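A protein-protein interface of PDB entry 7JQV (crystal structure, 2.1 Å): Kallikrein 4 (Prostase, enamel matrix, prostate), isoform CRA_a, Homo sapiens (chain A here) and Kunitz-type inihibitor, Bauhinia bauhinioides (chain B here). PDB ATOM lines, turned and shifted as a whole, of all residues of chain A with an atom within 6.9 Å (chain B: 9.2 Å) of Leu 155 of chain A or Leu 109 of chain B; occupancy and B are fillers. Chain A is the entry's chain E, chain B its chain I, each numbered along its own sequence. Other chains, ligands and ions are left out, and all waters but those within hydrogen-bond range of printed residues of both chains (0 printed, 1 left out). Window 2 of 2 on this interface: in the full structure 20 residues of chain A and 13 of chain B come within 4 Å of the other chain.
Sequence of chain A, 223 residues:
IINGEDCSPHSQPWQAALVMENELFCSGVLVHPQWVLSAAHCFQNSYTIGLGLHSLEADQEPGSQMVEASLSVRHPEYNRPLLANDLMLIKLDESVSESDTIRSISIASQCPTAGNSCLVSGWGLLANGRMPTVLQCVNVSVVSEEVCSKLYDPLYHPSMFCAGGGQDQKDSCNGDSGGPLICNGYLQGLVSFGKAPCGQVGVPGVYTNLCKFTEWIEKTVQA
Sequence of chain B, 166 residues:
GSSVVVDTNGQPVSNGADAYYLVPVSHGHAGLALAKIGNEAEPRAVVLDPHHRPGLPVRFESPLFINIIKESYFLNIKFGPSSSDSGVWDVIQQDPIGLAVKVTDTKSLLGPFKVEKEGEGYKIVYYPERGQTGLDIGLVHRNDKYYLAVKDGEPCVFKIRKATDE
The backbone carbonyl oxygen (O) of Pro 63 of chain B is in hydrogen-bond range of the backbone NH (N) of Gly 194 of chain A (3.0 Å).
Of the printed residues of chain B, Leu 82 of chain A touches Leu 110.
No residue of chain B comes within 4 Å of Pro 154 of chain A.
Of chain B, only Leu 109 (3.4 Å) comes within 4 Å of Leu 155 of chain A.
Printed residues of chain B within 4 Å of Phe 193 of chain A: Pro 63 (3.3 Å) and Leu 64 (3.9 Å).
Printed residues of chain A within 4 Å of Pro 63 of chain B: Phe 193 (3.3 Å) and Gly 194 (3.0 Å).
Of the printed residues of chain A, Leu 64 of chain B touches Phe 193.
Of the printed residues of chain A, Leu 109 of chain B touches Leu 155 (3.4 Å).
Of the printed residues of chain A, Leu 110 of chain B touches Leu 82 (3.9 Å).
The nearest residue of chain A that does not touch Leu 109 of chain B is Phe 193 of chain A (4.03 Å).
The nearest printed residue of chain A that does not touch Leu 110 of chain B is Leu 83 of chain A (4.1 Å).
Hydrophobic or aromatic side chains of chain A within 4 Å of the printed part of chain B: Leu 82, Leu 155 and Phe 193.
Among the printed residues, 5 pairs touch across the chains.
Among the printed residues, merely in contact across the chains: Phe 193 of chain A with Pro 63 of chain B (3.3 Å), Leu 155 of chain A with Leu 109 of chain B (3.4 Å), Phe 193 of chain A with Leu 64 of chain B (3.9 Å) and Leu 82 of chain A with Leu 110 of chain B (3.9 Å).
The backbone carbonyl oxygen (O) of Phe 193 of chain A is in hydrogen-bond range of the backbone NH (N) of Val 206 of chain A (2.7 Å).
O of Leu 64 of chain B sits at hydrogen-bond distance from ND2 of Asn 15 of chain B, at 3.1 Å.
N of Leu 64 of chain B sits close to OG of Ser 62 of chain B (3.2 Å).
The backbone carbonyl oxygen (O) of Leu 110 of chain B lies within hydrogen-bond range of the guanidinium group (NH1) of Arg 130 of chain B (2.9 Å).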
ATOM      1  N   PRO A  81     -19.436  25.464  -1.625  1.00  0.00           N
ATOM      2  CA  PRO A  81     -18.878  24.790  -2.811  1.00  0.00           C
ATOM      3  C   PRO A  81     -19.292  25.411  -4.170  1.00  0.00           C
ATOM      4  O   PRO A  81     -20.134  26.357  -4.269  1.00  0.00           O
ATOM      5  CB  PRO A  81     -19.411  23.332  -2.673  1.00  0.00           C
ATOM      6  CG  PRO A  81     -20.772  23.532  -1.952  1.00  0.00           C
ATOM      7  CD  PRO A  81     -20.553  24.743  -1.003  1.00  0.00           C
ATOM      8  N   LEU A  82     -18.649  24.952  -5.256  1.00  0.00           N
ATOM      9  CA  LEU A  82     -18.855  25.614  -6.568  1.00  0.00           C
ATOM     10  C   LEU A  82     -20.370  25.610  -6.821  1.00  0.00           C
ATOM     11  O   LEU A  82     -20.990  24.524  -6.683  1.00  0.00           O
ATOM     12  CB  LEU A  82     -18.137  24.812  -7.654  1.00  0.00           C
ATOM     13  CG  LEU A  82     -16.593  25.000  -7.569  1.00  0.00           C
ATOM     14  CD1 LEU A  82     -15.900  24.126  -8.595  1.00  0.00           C
ATOM     15  CD2 LEU A  82     -16.264  26.469  -7.814  1.00  0.00           C
ATOM     16  N   LEU A  83     -20.873  26.736  -7.353  1.00  0.00           N
ATOM     17  CA  LEU A  83     -22.268  26.984  -7.726  1.00  0.00           C
ATOM     18  C   LEU A  83     -23.181  27.248  -6.532  1.00  0.00           C
ATOM     19  O   LEU A  83     -24.342  27.652  -6.769  1.00  0.00           O
ATOM     20  CB  LEU A  83     -22.879  25.866  -8.575  1.00  0.00           C
ATOM     21  CG  LEU A  83     -22.086  25.469  -9.834  1.00  0.00           C
ATOM     22  CD1 LEU A  83     -22.736  24.230 -10.486  1.00  0.00           C
ATOM     23  CD2 LEU A  83     -21.925  26.634 -10.834  1.00  0.00           C
ATOM     24  N   ALA A  84     -22.704  27.066  -5.277  1.00  0.00           N
ATOM     25  CA  ALA A  84     -23.610  27.125  -4.137  1.00  0.00           C
ATOM     26  C   ALA A  84     -23.835  28.550  -3.678  1.00  0.00           C
ATOM     27  O   ALA A  84     -23.025  29.405  -4.014  1.00  0.00           O
ATOM     28  CB  ALA A  84     -23.087  26.320  -2.946  1.00  0.00           C
ATOM     29  N   SER A 149     -30.391  15.574  -5.353  1.00  0.00           N
ATOM     30  CA  SER A 149     -29.017  15.192  -5.009  1.00  0.00           C
ATOM     31  C   SER A 149     -28.633  14.030  -5.911  1.00  0.00           C
ATOM     32  O   SER A 149     -27.498  13.923  -6.378  1.00  0.00           O
ATOM     33  CB  SER A 149     -28.977  14.800  -3.545  1.00  0.00           C
ATOM     34  OG  SER A 149     -29.719  13.625  -3.405  1.00  0.00           O
ATOM     35  N   LEU A 151     -29.435  13.558  -8.999  1.00  0.00           N
ATOM     36  CA  LEU A 151     -29.023  14.009 -10.333  1.00  0.00           C
ATOM     37  C   LEU A 151     -27.820  14.965 -10.245  1.00  0.00           C
ATOM     38  O   LEU A 151     -27.057  15.099 -11.213  1.00  0.00           O
ATOM     39  CB  LEU A 151     -30.213  14.738 -10.964  1.00  0.00           C
ATOM     40  CG  LEU A 151     -31.472  13.870 -11.083  1.00  0.00           C
ATOM     41  CD1 LEU A 151     -32.564  14.675 -11.769  1.00  0.00           C
ATOM     42  CD2 LEU A 151     -31.187  12.571 -11.861  1.00  0.00           C
ATOM     43  N   TYR A 152     -27.649  15.699  -9.126  1.00  0.00           N
ATOM     44  CA  TYR A 152     -26.644  16.765  -9.205  1.00  0.00           C
ATOM     45  C   TYR A 152     -25.435  16.524  -8.284  1.00  0.00           C
ATOM     46  O   TYR A 152     -24.474  17.277  -8.396  1.00  0.00           O
ATOM     47  CB  TYR A 152     -27.259  18.166  -8.950  1.00  0.00           C
ATOM     48  CG  TYR A 152     -27.974  18.765 -10.163  1.00  0.00           C
ATOM     49  CD1 TYR A 152     -27.273  19.327 -11.243  1.00  0.00           C
ATOM     50  CD2 TYR A 152     -29.358  18.644 -10.297  1.00  0.00           C
ATOM     51  CE1 TYR A 152     -27.917  19.820 -12.372  1.00  0.00           C
ATOM     52  CE2 TYR A 152     -30.031  19.185 -11.398  1.00  0.00           C
ATOM     53  CZ  TYR A 152     -29.307  19.765 -12.437  1.00  0.00           C
ATOM     54  OH  TYR A 152     -29.970  20.259 -13.525  1.00  0.00           O
ATOM     55  N   ASP A 153     -25.500  15.625  -7.281  1.00  0.00           N
ATOM     56  CA  ASP A 153     -24.282  15.351  -6.501  1.00  0.00           C
ATOM     57  C   ASP A 153     -23.125  15.075  -7.460  1.00  0.00           C
ATOM     58  O   ASP A 153     -23.355  14.385  -8.432  1.00  0.00           O
ATOM     59  CB  ASP A 153     -24.416  14.039  -5.770  1.00  0.00           C
ATOM     60  CG  ASP A 153     -25.145  14.232  -4.437  1.00  0.00           C
ATOM     61  OD1 ASP A 153     -25.496  15.370  -4.080  1.00  0.00           O
ATOM     62  OD2 ASP A 153     -25.425  13.257  -3.805  1.00  0.00           O
ATOM     63  N   PRO A 154     -21.862  15.518  -7.225  1.00  0.00           N
ATOM     64  CA  PRO A 154     -21.456  16.098  -5.941  1.00  0.00           C
ATOM     65  C   PRO A 154     -21.637  17.605  -5.779  1.00  0.00           C
ATOM     66  O   PRO A 154     -21.012  18.199  -4.872  1.00  0.00           O
ATOM     67  CB  PRO A 154     -19.920  15.801  -5.851  1.00  0.00           C
ATOM     68  CG  PRO A 154     -19.504  15.886  -7.342  1.00  0.00           C
ATOM     69  CD  PRO A 154     -20.719  15.324  -8.145  1.00  0.00           C
ATOM     70  N   LEU A 155     -22.404  18.238  -6.691  1.00  0.00           N
ATOM     71  CA  LEU A 155     -22.573  19.686  -6.687  1.00  0.00           C
ATOM     72  C   LEU A 155     -23.919  20.110  -6.067  1.00  0.00           C
ATOM     73  O   LEU A 155     -24.198  21.299  -5.960  1.00  0.00           O
ATOM     74  CB  LEU A 155     -22.416  20.192  -8.120  1.00  0.00           C
ATOM     75  CG  LEU A 155     -21.001  20.013  -8.689  1.00  0.00           C
ATOM     76  CD1 LEU A 155     -20.953  20.501 -10.128  1.00  0.00           C
ATOM     77  CD2 LEU A 155     -20.030  20.844  -7.889  1.00  0.00           C
ATOM     78  N   TYR A 156     -24.764  19.156  -5.677  1.00  0.00           N
ATOM     79  CA  TYR A 156     -25.968  19.489  -4.893  1.00  0.00           C
ATOM     80  C   TYR A 156     -25.568  19.966  -3.488  1.00  0.00           C
ATOM     81  O   TYR A 156     -24.879  19.292  -2.710  1.00  0.00           O
ATOM     82  CB  TYR A 156     -26.964  18.324  -4.816  1.00  0.00           C
ATOM     83  CG  TYR A 156     -28.044  18.652  -3.808  1.00  0.00           C
ATOM     84  CD1 TYR A 156     -29.010  19.630  -4.116  1.00  0.00           C
ATOM     85  CD2 TYR A 156     -27.976  18.155  -2.494  1.00  0.00           C
ATOM     86  CE1 TYR A 156     -29.959  20.022  -3.162  1.00  0.00           C
ATOM     87  CE2 TYR A 156     -28.895  18.592  -1.510  1.00  0.00           C
ATOM     88  CZ  TYR A 156     -29.893  19.493  -1.859  1.00  0.00           C
ATOM     89  OH  TYR A 156     -30.795  19.878  -0.898  1.00  0.00           O
ATOM     90  N   HIS A 157     -26.051  21.147  -3.119  1.00  0.00           N
ATOM     91  CA  HIS A 157     -25.894  21.705  -1.783  1.00  0.00           C
ATOM     92  C   HIS A 157     -27.256  22.287  -1.298  1.00  0.00           C
ATOM     93  O   HIS A 157     -28.064  22.765  -2.101  1.00  0.00           O
ATOM     94  CB  HIS A 157     -24.816  22.806  -1.905  1.00  0.00           C
ATOM     95  CG  HIS A 157     -24.500  23.473  -0.598  1.00  0.00           C
ATOM     96  ND1 HIS A 157     -24.974  24.735  -0.242  1.00  0.00           N
ATOM     97  CD2 HIS A 157     -23.632  23.079   0.401  1.00  0.00           C
ATOM     98  CE1 HIS A 157     -24.444  25.094   0.943  1.00  0.00           C
ATOM     99  NE2 HIS A 157     -23.625  24.083   1.350  1.00  0.00           N
ATOM    100  N   MET A 160     -29.506  25.103  -2.633  1.00  0.00           N
ATOM    101  CA  MET A 160     -30.159  24.934  -3.927  1.00  0.00           C
ATOM    102  C   MET A 160     -31.378  24.032  -3.750  1.00  0.00           C
ATOM    103  O   MET A 160     -31.447  23.272  -2.810  1.00  0.00           O
ATOM    104  CB  MET A 160     -29.255  24.071  -4.813  1.00  0.00           C
ATOM    105  CG  MET A 160     -27.794  24.699  -4.948  1.00  0.00           C
ATOM    106  SD  MET A 160     -26.787  23.352  -5.703  1.00  0.00           S
ATOM    107  CE  MET A 160     -25.234  24.238  -5.859  1.00  0.00           C
ATOM    108  N   PHE A 193     -28.994  27.563 -12.198  1.00  0.00           N
ATOM    109  CA  PHE A 193     -28.208  26.751 -13.115  1.00  0.00           C
ATOM    110  C   PHE A 193     -28.906  25.427 -13.459  1.00  0.00           C
ATOM    111  O   PHE A 193     -29.870  25.042 -12.817  1.00  0.00           O
ATOM    112  CB  PHE A 193     -26.751  26.501 -12.658  1.00  0.00           C
ATOM    113  CG  PHE A 193     -26.619  25.485 -11.554  1.00  0.00           C
ATOM    114  CD1 PHE A 193     -26.719  25.871 -10.220  1.00  0.00           C
ATOM    115  CD2 PHE A 193     -26.507  24.113 -11.862  1.00  0.00           C
ATOM    116  CE1 PHE A 193     -26.524  24.901  -9.228  1.00  0.00           C
ATOM    117  CE2 PHE A 193     -26.335  23.138 -10.877  1.00  0.00           C
ATOM    118  CZ  PHE A 193     -26.369  23.541  -9.542  1.00  0.00           C
ATOM    119  N   GLY A 194     -28.494  24.778 -14.564  1.00  0.00           N
ATOM    120  CA  GLY A 194     -28.999  23.436 -14.881  1.00  0.00           C
ATOM    121  C   GLY A 194     -28.044  22.723 -15.839  1.00  0.00           C
ATOM    122  O   GLY A 194     -27.155  23.399 -16.365  1.00  0.00           O
ATOM    123  N   LYS A 195     -28.304  21.454 -16.178  1.00  0.00           N
ATOM    124  CA  LYS A 195     -27.505  20.833 -17.249  1.00  0.00           C
ATOM    125  C   LYS A 195     -28.168  21.077 -18.602  1.00  0.00           C
ATOM    126  O   LYS A 195     -29.364  20.855 -18.724  1.00  0.00           O
ATOM    127  CB  LYS A 195     -27.272  19.320 -17.155  1.00  0.00           C
ATOM    128  CG  LYS A 195     -27.782  18.595 -15.920  1.00  0.00           C
ATOM    129  CD  LYS A 195     -27.475  17.085 -15.857  1.00  0.00           C
ATOM    130  CE  LYS A 195     -27.406  16.550 -14.431  1.00  0.00           C
ATOM    131  NZ  LYS A 195     -28.056  15.225 -14.264  1.00  0.00           N
ATOM    132  N   ALA A 196     -27.393  21.578 -19.583  1.00  0.00           N
ATOM    133  CA  ALA A 196     -27.789  21.914 -20.959  1.00  0.00           C
ATOM    134  C   ALA A 196     -28.227  20.664 -21.730  1.00  0.00           C
ATOM    135  O   ALA A 196     -27.898  19.528 -21.401  1.00  0.00           O
ATOM    136  CB  ALA A 196     -26.632  22.593 -21.674  1.00  0.00           C
ATOM    137  N   VAL A 206     -32.027  24.197 -11.342  1.00  0.00           N
ATOM    138  CA  VAL A 206     -31.620  24.398  -9.976  1.00  0.00           C
ATOM    139  C   VAL A 206     -31.783  25.880  -9.637  1.00  0.00           C
ATOM    140  O   VAL A 206     -31.453  26.701 -10.430  1.00  0.00           O
ATOM    141  CB  VAL A 206     -30.161  23.926  -9.756  1.00  0.00           C
ATOM    142  CG1 VAL A 206     -29.827  23.940  -8.258  1.00  0.00           C
ATOM    143  CG2 VAL A 206     -30.019  22.521 -10.332  1.00  0.00           C
ATOM    144  N   ASN B  15     -23.286  32.142 -24.079  1.00  0.00           N
ATOM    145  CA  ASN B  15     -23.127  30.926 -23.316  1.00  0.00           C
ATOM    146  C   ASN B  15     -23.729  29.841 -24.164  1.00  0.00           C
ATOM    147  O   ASN B  15     -24.918  29.664 -24.133  1.00  0.00           O
ATOM    148  CB  ASN B  15     -23.843  31.041 -21.950  1.00  0.00           C
ATOM    149  CG  ASN B  15     -23.797  29.778 -21.133  1.00  0.00           C
ATOM    150  OD1 ASN B  15     -23.129  28.798 -21.553  1.00  0.00           O
ATOM    151  ND2 ASN B  15     -24.433  29.793 -19.937  1.00  0.00           N
ATOM    152  N   GLU B  61     -19.373  26.959 -22.797  1.00  0.00           N
ATOM    153  CA  GLU B  61     -20.628  26.680 -22.110  1.00  0.00           C
ATOM    154  C   GLU B  61     -20.432  26.656 -20.596  1.00  0.00           C
ATOM    155  O   GLU B  61     -19.473  26.022 -20.103  1.00  0.00           O
ATOM    156  CB  GLU B  61     -21.037  25.230 -22.384  1.00  0.00           C
ATOM    157  CG  GLU B  61     -21.674  24.917 -23.687  1.00  0.00           C
ATOM    158  CD  GLU B  61     -22.272  23.505 -23.650  1.00  0.00           C
ATOM    159  OE1 GLU B  61     -22.682  22.962 -22.566  1.00  0.00           O
ATOM    160  OE2 GLU B  61     -22.326  22.937 -24.722  1.00  0.00           O
ATOM    161  N   SER B  62     -21.427  27.234 -19.902  1.00  0.00           N
ATOM    162  CA  SER B  62     -21.489  27.229 -18.445  1.00  0.00           C
ATOM    163  C   SER B  62     -22.867  26.672 -18.034  1.00  0.00           C
ATOM    164  O   SER B  62     -23.880  26.913 -18.730  1.00  0.00           O
ATOM    165  CB  SER B  62     -21.343  28.651 -17.943  1.00  0.00           C
ATOM    166  OG  SER B  62     -21.698  28.741 -16.525  1.00  0.00           O
ATOM    167  N   PRO B  63     -23.020  25.911 -16.920  1.00  0.00           N
ATOM    168  CA  PRO B  63     -24.382  25.487 -16.542  1.00  0.00           C
ATOM    169  C   PRO B  63     -25.274  26.651 -16.109  1.00  0.00           C
ATOM    170  O   PRO B  63     -26.466  26.411 -15.957  1.00  0.00           O
ATOM    171  CB  PRO B  63     -24.113  24.479 -15.398  1.00  0.00           C
ATOM    172  CG  PRO B  63     -22.792  24.962 -14.741  1.00  0.00           C
ATOM    173  CD  PRO B  63     -21.984  25.470 -15.930  1.00  0.00           C
ATOM    174  N   LEU B  64     -24.699  27.828 -15.726  1.00  0.00           N
ATOM    175  CA  LEU B  64     -25.436  29.004 -15.274  1.00  0.00           C
ATOM    176  C   LEU B  64     -26.502  29.413 -16.298  1.00  0.00           C
ATOM    177  O   LEU B  64     -26.286  29.430 -17.516  1.00  0.00           O
ATOM    178  CB  LEU B  64     -24.444  30.153 -14.972  1.00  0.00           C
ATOM    179  CG  LEU B  64     -23.346  29.846 -13.902  1.00  0.00           C
ATOM    180  CD1 LEU B  64     -22.320  30.951 -13.901  1.00  0.00           C
ATOM    181  CD2 LEU B  64     -23.943  29.698 -12.474  1.00  0.00           C
ATOM    182  N   PHE B  74     -16.073  28.753 -14.676  1.00  0.00           N
ATOM    183  CA  PHE B  74     -15.627  27.494 -15.277  1.00  0.00           C
ATOM    184  C   PHE B  74     -16.442  27.156 -16.522  1.00  0.00           C
ATOM    185  O   PHE B  74     -17.677  27.134 -16.427  1.00  0.00           O
ATOM    186  CB  PHE B  74     -15.688  26.336 -14.280  1.00  0.00           C
ATOM    187  CG  PHE B  74     -14.558  26.347 -13.267  1.00  0.00           C
ATOM    188  CD1 PHE B  74     -13.244  26.165 -13.700  1.00  0.00           C
ATOM    189  CD2 PHE B  74     -14.792  26.587 -11.906  1.00  0.00           C
ATOM    190  CE1 PHE B  74     -12.212  26.128 -12.772  1.00  0.00           C
ATOM    191  CE2 PHE B  74     -13.741  26.669 -10.979  1.00  0.00           C
ATOM    192  CZ  PHE B  74     -12.460  26.382 -11.427  1.00  0.00           C
ATOM    193  N   LEU B  75     -15.751  26.763 -17.619  1.00  0.00           N
ATOM    194  CA  LEU B  75     -16.373  26.562 -18.949  1.00  0.00           C
ATOM    195  C   LEU B  75     -15.989  25.207 -19.507  1.00  0.00           C
ATOM    196  O   LEU B  75     -14.902  24.711 -19.236  1.00  0.00           O
ATOM    197  CB  LEU B  75     -15.894  27.608 -19.977  1.00  0.00           C
ATOM    198  CG  LEU B  75     -16.116  29.080 -19.630  1.00  0.00           C
ATOM    199  CD1 LEU B  75     -15.404  29.977 -20.598  1.00  0.00           C
ATOM    200  CD2 LEU B  75     -17.551  29.531 -19.484  1.00  0.00           C
ATOM    201  N   ASN B  76     -16.950  24.559 -20.189  1.00  0.00           N
ATOM    202  CA  ASN B  76     -16.602  23.563 -21.182  1.00  0.00           C
ATOM    203  C   ASN B  76     -16.372  24.328 -22.488  1.00  0.00           C
ATOM    204  O   ASN B  76     -16.963  25.412 -22.736  1.00  0.00           O
ATOM    205  CB  ASN B  76     -17.745  22.533 -21.457  1.00  0.00           C
ATOM    206  CG  ASN B  76     -17.715  21.458 -20.411  1.00  0.00           C
ATOM    207  OD1 ASN B  76     -16.697  20.788 -20.199  1.00  0.00           O
ATOM    208  ND2 ASN B  76     -18.760  21.448 -19.601  1.00  0.00           N
ATOM    209  N   ASP B  85     -22.265  16.514 -27.936  1.00  0.00           N
ATOM    210  CA  ASP B  85     -21.154  16.505 -27.001  1.00  0.00           C
ATOM    211  C   ASP B  85     -20.042  15.627 -27.536  1.00  0.00           C
ATOM    212  O   ASP B  85     -19.274  15.126 -26.730  1.00  0.00           O
ATOM    213  CB  ASP B  85     -21.511  16.125 -25.564  1.00  0.00           C
ATOM    214  CG  ASP B  85     -22.522  17.051 -24.875  1.00  0.00           C
ATOM    215  OD1 ASP B  85     -22.691  18.219 -25.300  1.00  0.00           O
ATOM    216  OD2 ASP B  85     -23.143  16.598 -23.895  1.00  0.00           O
ATOM    217  N   VAL B  88     -15.995  17.860 -27.088  1.00  0.00           N
ATOM    218  CA  VAL B  88     -15.676  18.445 -25.791  1.00  0.00           C
ATOM    219  C   VAL B  88     -14.193  18.391 -25.462  1.00  0.00           C
ATOM    220  O   VAL B  88     -13.582  17.330 -25.514  1.00  0.00           O
ATOM    221  CB  VAL B  88     -16.517  17.779 -24.680  1.00  0.00           C
ATOM    222  CG1 VAL B  88     -16.273  18.472 -23.348  1.00  0.00           C
ATOM    223  CG2 VAL B  88     -17.997  17.872 -25.045  1.00  0.00           C
ATOM    224  N   THR B 106     -17.676  13.004 -23.736  1.00  0.00           N
ATOM    225  CA  THR B 106     -18.394  13.200 -22.484  1.00  0.00           C
ATOM    226  C   THR B 106     -18.087  14.593 -21.920  1.00  0.00           C
ATOM    227  O   THR B 106     -16.981  15.073 -22.037  1.00  0.00           O
ATOM    228  CB  THR B 106     -17.983  12.109 -21.486  1.00  0.00           C
ATOM    229  OG1 THR B 106     -16.561  12.237 -21.356  1.00  0.00           O
ATOM    230  CG2 THR B 106     -18.392  10.724 -21.960  1.00  0.00           C
ATOM    231  N   LYS B 107     -19.068  15.225 -21.281  1.00  0.00           N
ATOM    232  CA  LYS B 107     -18.976  16.549 -20.703  1.00  0.00           C
ATOM    233  C   LYS B 107     -19.318  16.465 -19.208  1.00  0.00           C
ATOM    234  O   LYS B 107     -20.311  15.848 -18.829  1.00  0.00           O
ATOM    235  CB  LYS B 107     -20.084  17.271 -21.455  1.00  0.00           C
ATOM    236  CG  LYS B 107     -20.222  18.749 -21.203  1.00  0.00           C
ATOM    237  CD  LYS B 107     -21.135  19.220 -22.248  1.00  0.00           C
ATOM    238  CE  LYS B 107     -22.507  19.575 -21.766  1.00  0.00           C
ATOM    239  NZ  LYS B 107     -23.298  20.073 -22.916  1.00  0.00           N
ATOM    240  N   SER B 108     -18.533  17.069 -18.332  1.00  0.00           N
ATOM    241  CA  SER B 108     -19.015  17.270 -16.958  1.00  0.00           C
ATOM    242  C   SER B 108     -19.947  18.473 -16.920  1.00  0.00           C
ATOM    243  O   SER B 108     -19.908  19.313 -17.806  1.00  0.00           O
ATOM    244  CB  SER B 108     -17.888  17.572 -16.007  1.00  0.00           C
ATOM    245  OG  SER B 108     -17.025  16.452 -16.007  1.00  0.00           O
ATOM    246  N   LEU B 109     -20.672  18.608 -15.811  1.00  0.00           N
ATOM    247  CA  LEU B 109     -21.554  19.734 -15.599  1.00  0.00           C
ATOM    248  C   LEU B 109     -20.707  21.013 -15.609  1.00  0.00           C
ATOM    249  O   LEU B 109     -21.137  22.003 -16.149  1.00  0.00           O
ATOM    250  CB  LEU B 109     -22.177  19.558 -14.209  1.00  0.00           C
ATOM    251  CG  LEU B 109     -23.122  20.713 -13.820  1.00  0.00           C
ATOM    252  CD1 LEU B 109     -24.332  20.719 -14.687  1.00  0.00           C
ATOM    253  CD2 LEU B 109     -23.521  20.664 -12.373  1.00  0.00           C
ATOM    254  N   LEU B 110     -19.554  21.030 -14.907  1.00  0.00           N
ATOM    255  CA  LEU B 110     -18.701  22.208 -14.939  1.00  0.00           C
ATOM    256  C   LEU B 110     -17.440  21.819 -15.690  1.00  0.00           C
ATOM    257  O   LEU B 110     -16.802  20.857 -15.287  1.00  0.00           O
ATOM    258  CB  LEU B 110     -18.263  22.590 -13.515  1.00  0.00           C
ATOM    259  CG  LEU B 110     -19.179  23.530 -12.758  1.00  0.00           C
ATOM    260  CD1 LEU B 110     -18.580  23.791 -11.387  1.00  0.00           C
ATOM    261  CD2 LEU B 110     -19.369  24.834 -13.508  1.00  0.00           C
ATOM    262  N   GLY B 111     -17.051  22.566 -16.727  1.00  0.00           N
ATOM    263  CA  GLY B 111     -15.809  22.185 -17.397  1.00  0.00           C
ATOM    264  C   GLY B 111     -14.608  22.782 -16.647  1.00  0.00           C
ATOM    265  O   GLY B 111     -14.781  23.522 -15.662  1.00  0.00           O
ATOM    266  N   PRO B 112     -13.370  22.449 -17.064  1.00  0.00           N
ATOM    267  CA  PRO B 112     -12.180  22.916 -16.331  1.00  0.00           C
ATOM    268  C   PRO B 112     -11.397  24.081 -16.906  1.00  0.00           C
ATOM    269  O   PRO B 112     -10.309  24.386 -16.403  1.00  0.00           O
ATOM    270  CB  PRO B 112     -11.325  21.641 -16.431  1.00  0.00           C
ATOM    271  CG  PRO B 112     -11.569  21.178 -17.866  1.00  0.00           C
ATOM    272  CD  PRO B 112     -13.075  21.379 -18.059  1.00  0.00           C
ATOM    273  N   GLU B 129      -8.687  19.682 -11.535  1.00  0.00           N
ATOM    274  CA  GLU B 129      -9.602  19.515 -10.401  1.00  0.00           C
ATOM    275  C   GLU B 129     -10.538  20.720 -10.212  1.00  0.00           C
ATOM    276  O   GLU B 129     -11.279  20.727  -9.229  1.00  0.00           O
ATOM    277  CB  GLU B 129      -8.855  19.483  -9.046  1.00  0.00           C
ATOM    278  CG  GLU B 129      -7.526  18.724  -8.937  1.00  0.00           C
ATOM    279  CD  GLU B 129      -7.749  17.326  -8.394  1.00  0.00           C
ATOM    280  OE1 GLU B 129      -8.133  16.557  -9.292  1.00  0.00           O
ATOM    281  OE2 GLU B 129      -7.635  17.031  -7.070  1.00  0.00           O
ATOM    282  N   ARG B 130     -10.518  21.730 -11.098  1.00  0.00           N
ATOM    283  CA  ARG B 130     -11.356  22.918 -10.945  1.00  0.00           C
ATOM    284  C   ARG B 130     -10.986  23.573  -9.597  1.00  0.00           C
ATOM    285  O   ARG B 130     -11.859  24.145  -8.948  1.00  0.00           O
ATOM    286  CB  ARG B 130     -12.870  22.605 -10.837  1.00  0.00           C
ATOM    287  CG  ARG B 130     -13.595  22.376 -12.161  1.00  0.00           C
ATOM    288  CD  ARG B 130     -13.227  21.017 -12.619  1.00  0.00           C
ATOM    289  NE  ARG B 130     -14.065  20.605 -13.726  1.00  0.00           N
ATOM    290  CZ  ARG B 130     -13.686  19.612 -14.510  1.00  0.00           C
ATOM    291  NH1 ARG B 130     -14.425  19.241 -15.529  1.00  0.00           N
ATOM    292  NH2 ARG B 130     -12.513  19.029 -14.307  1.00  0.00           N
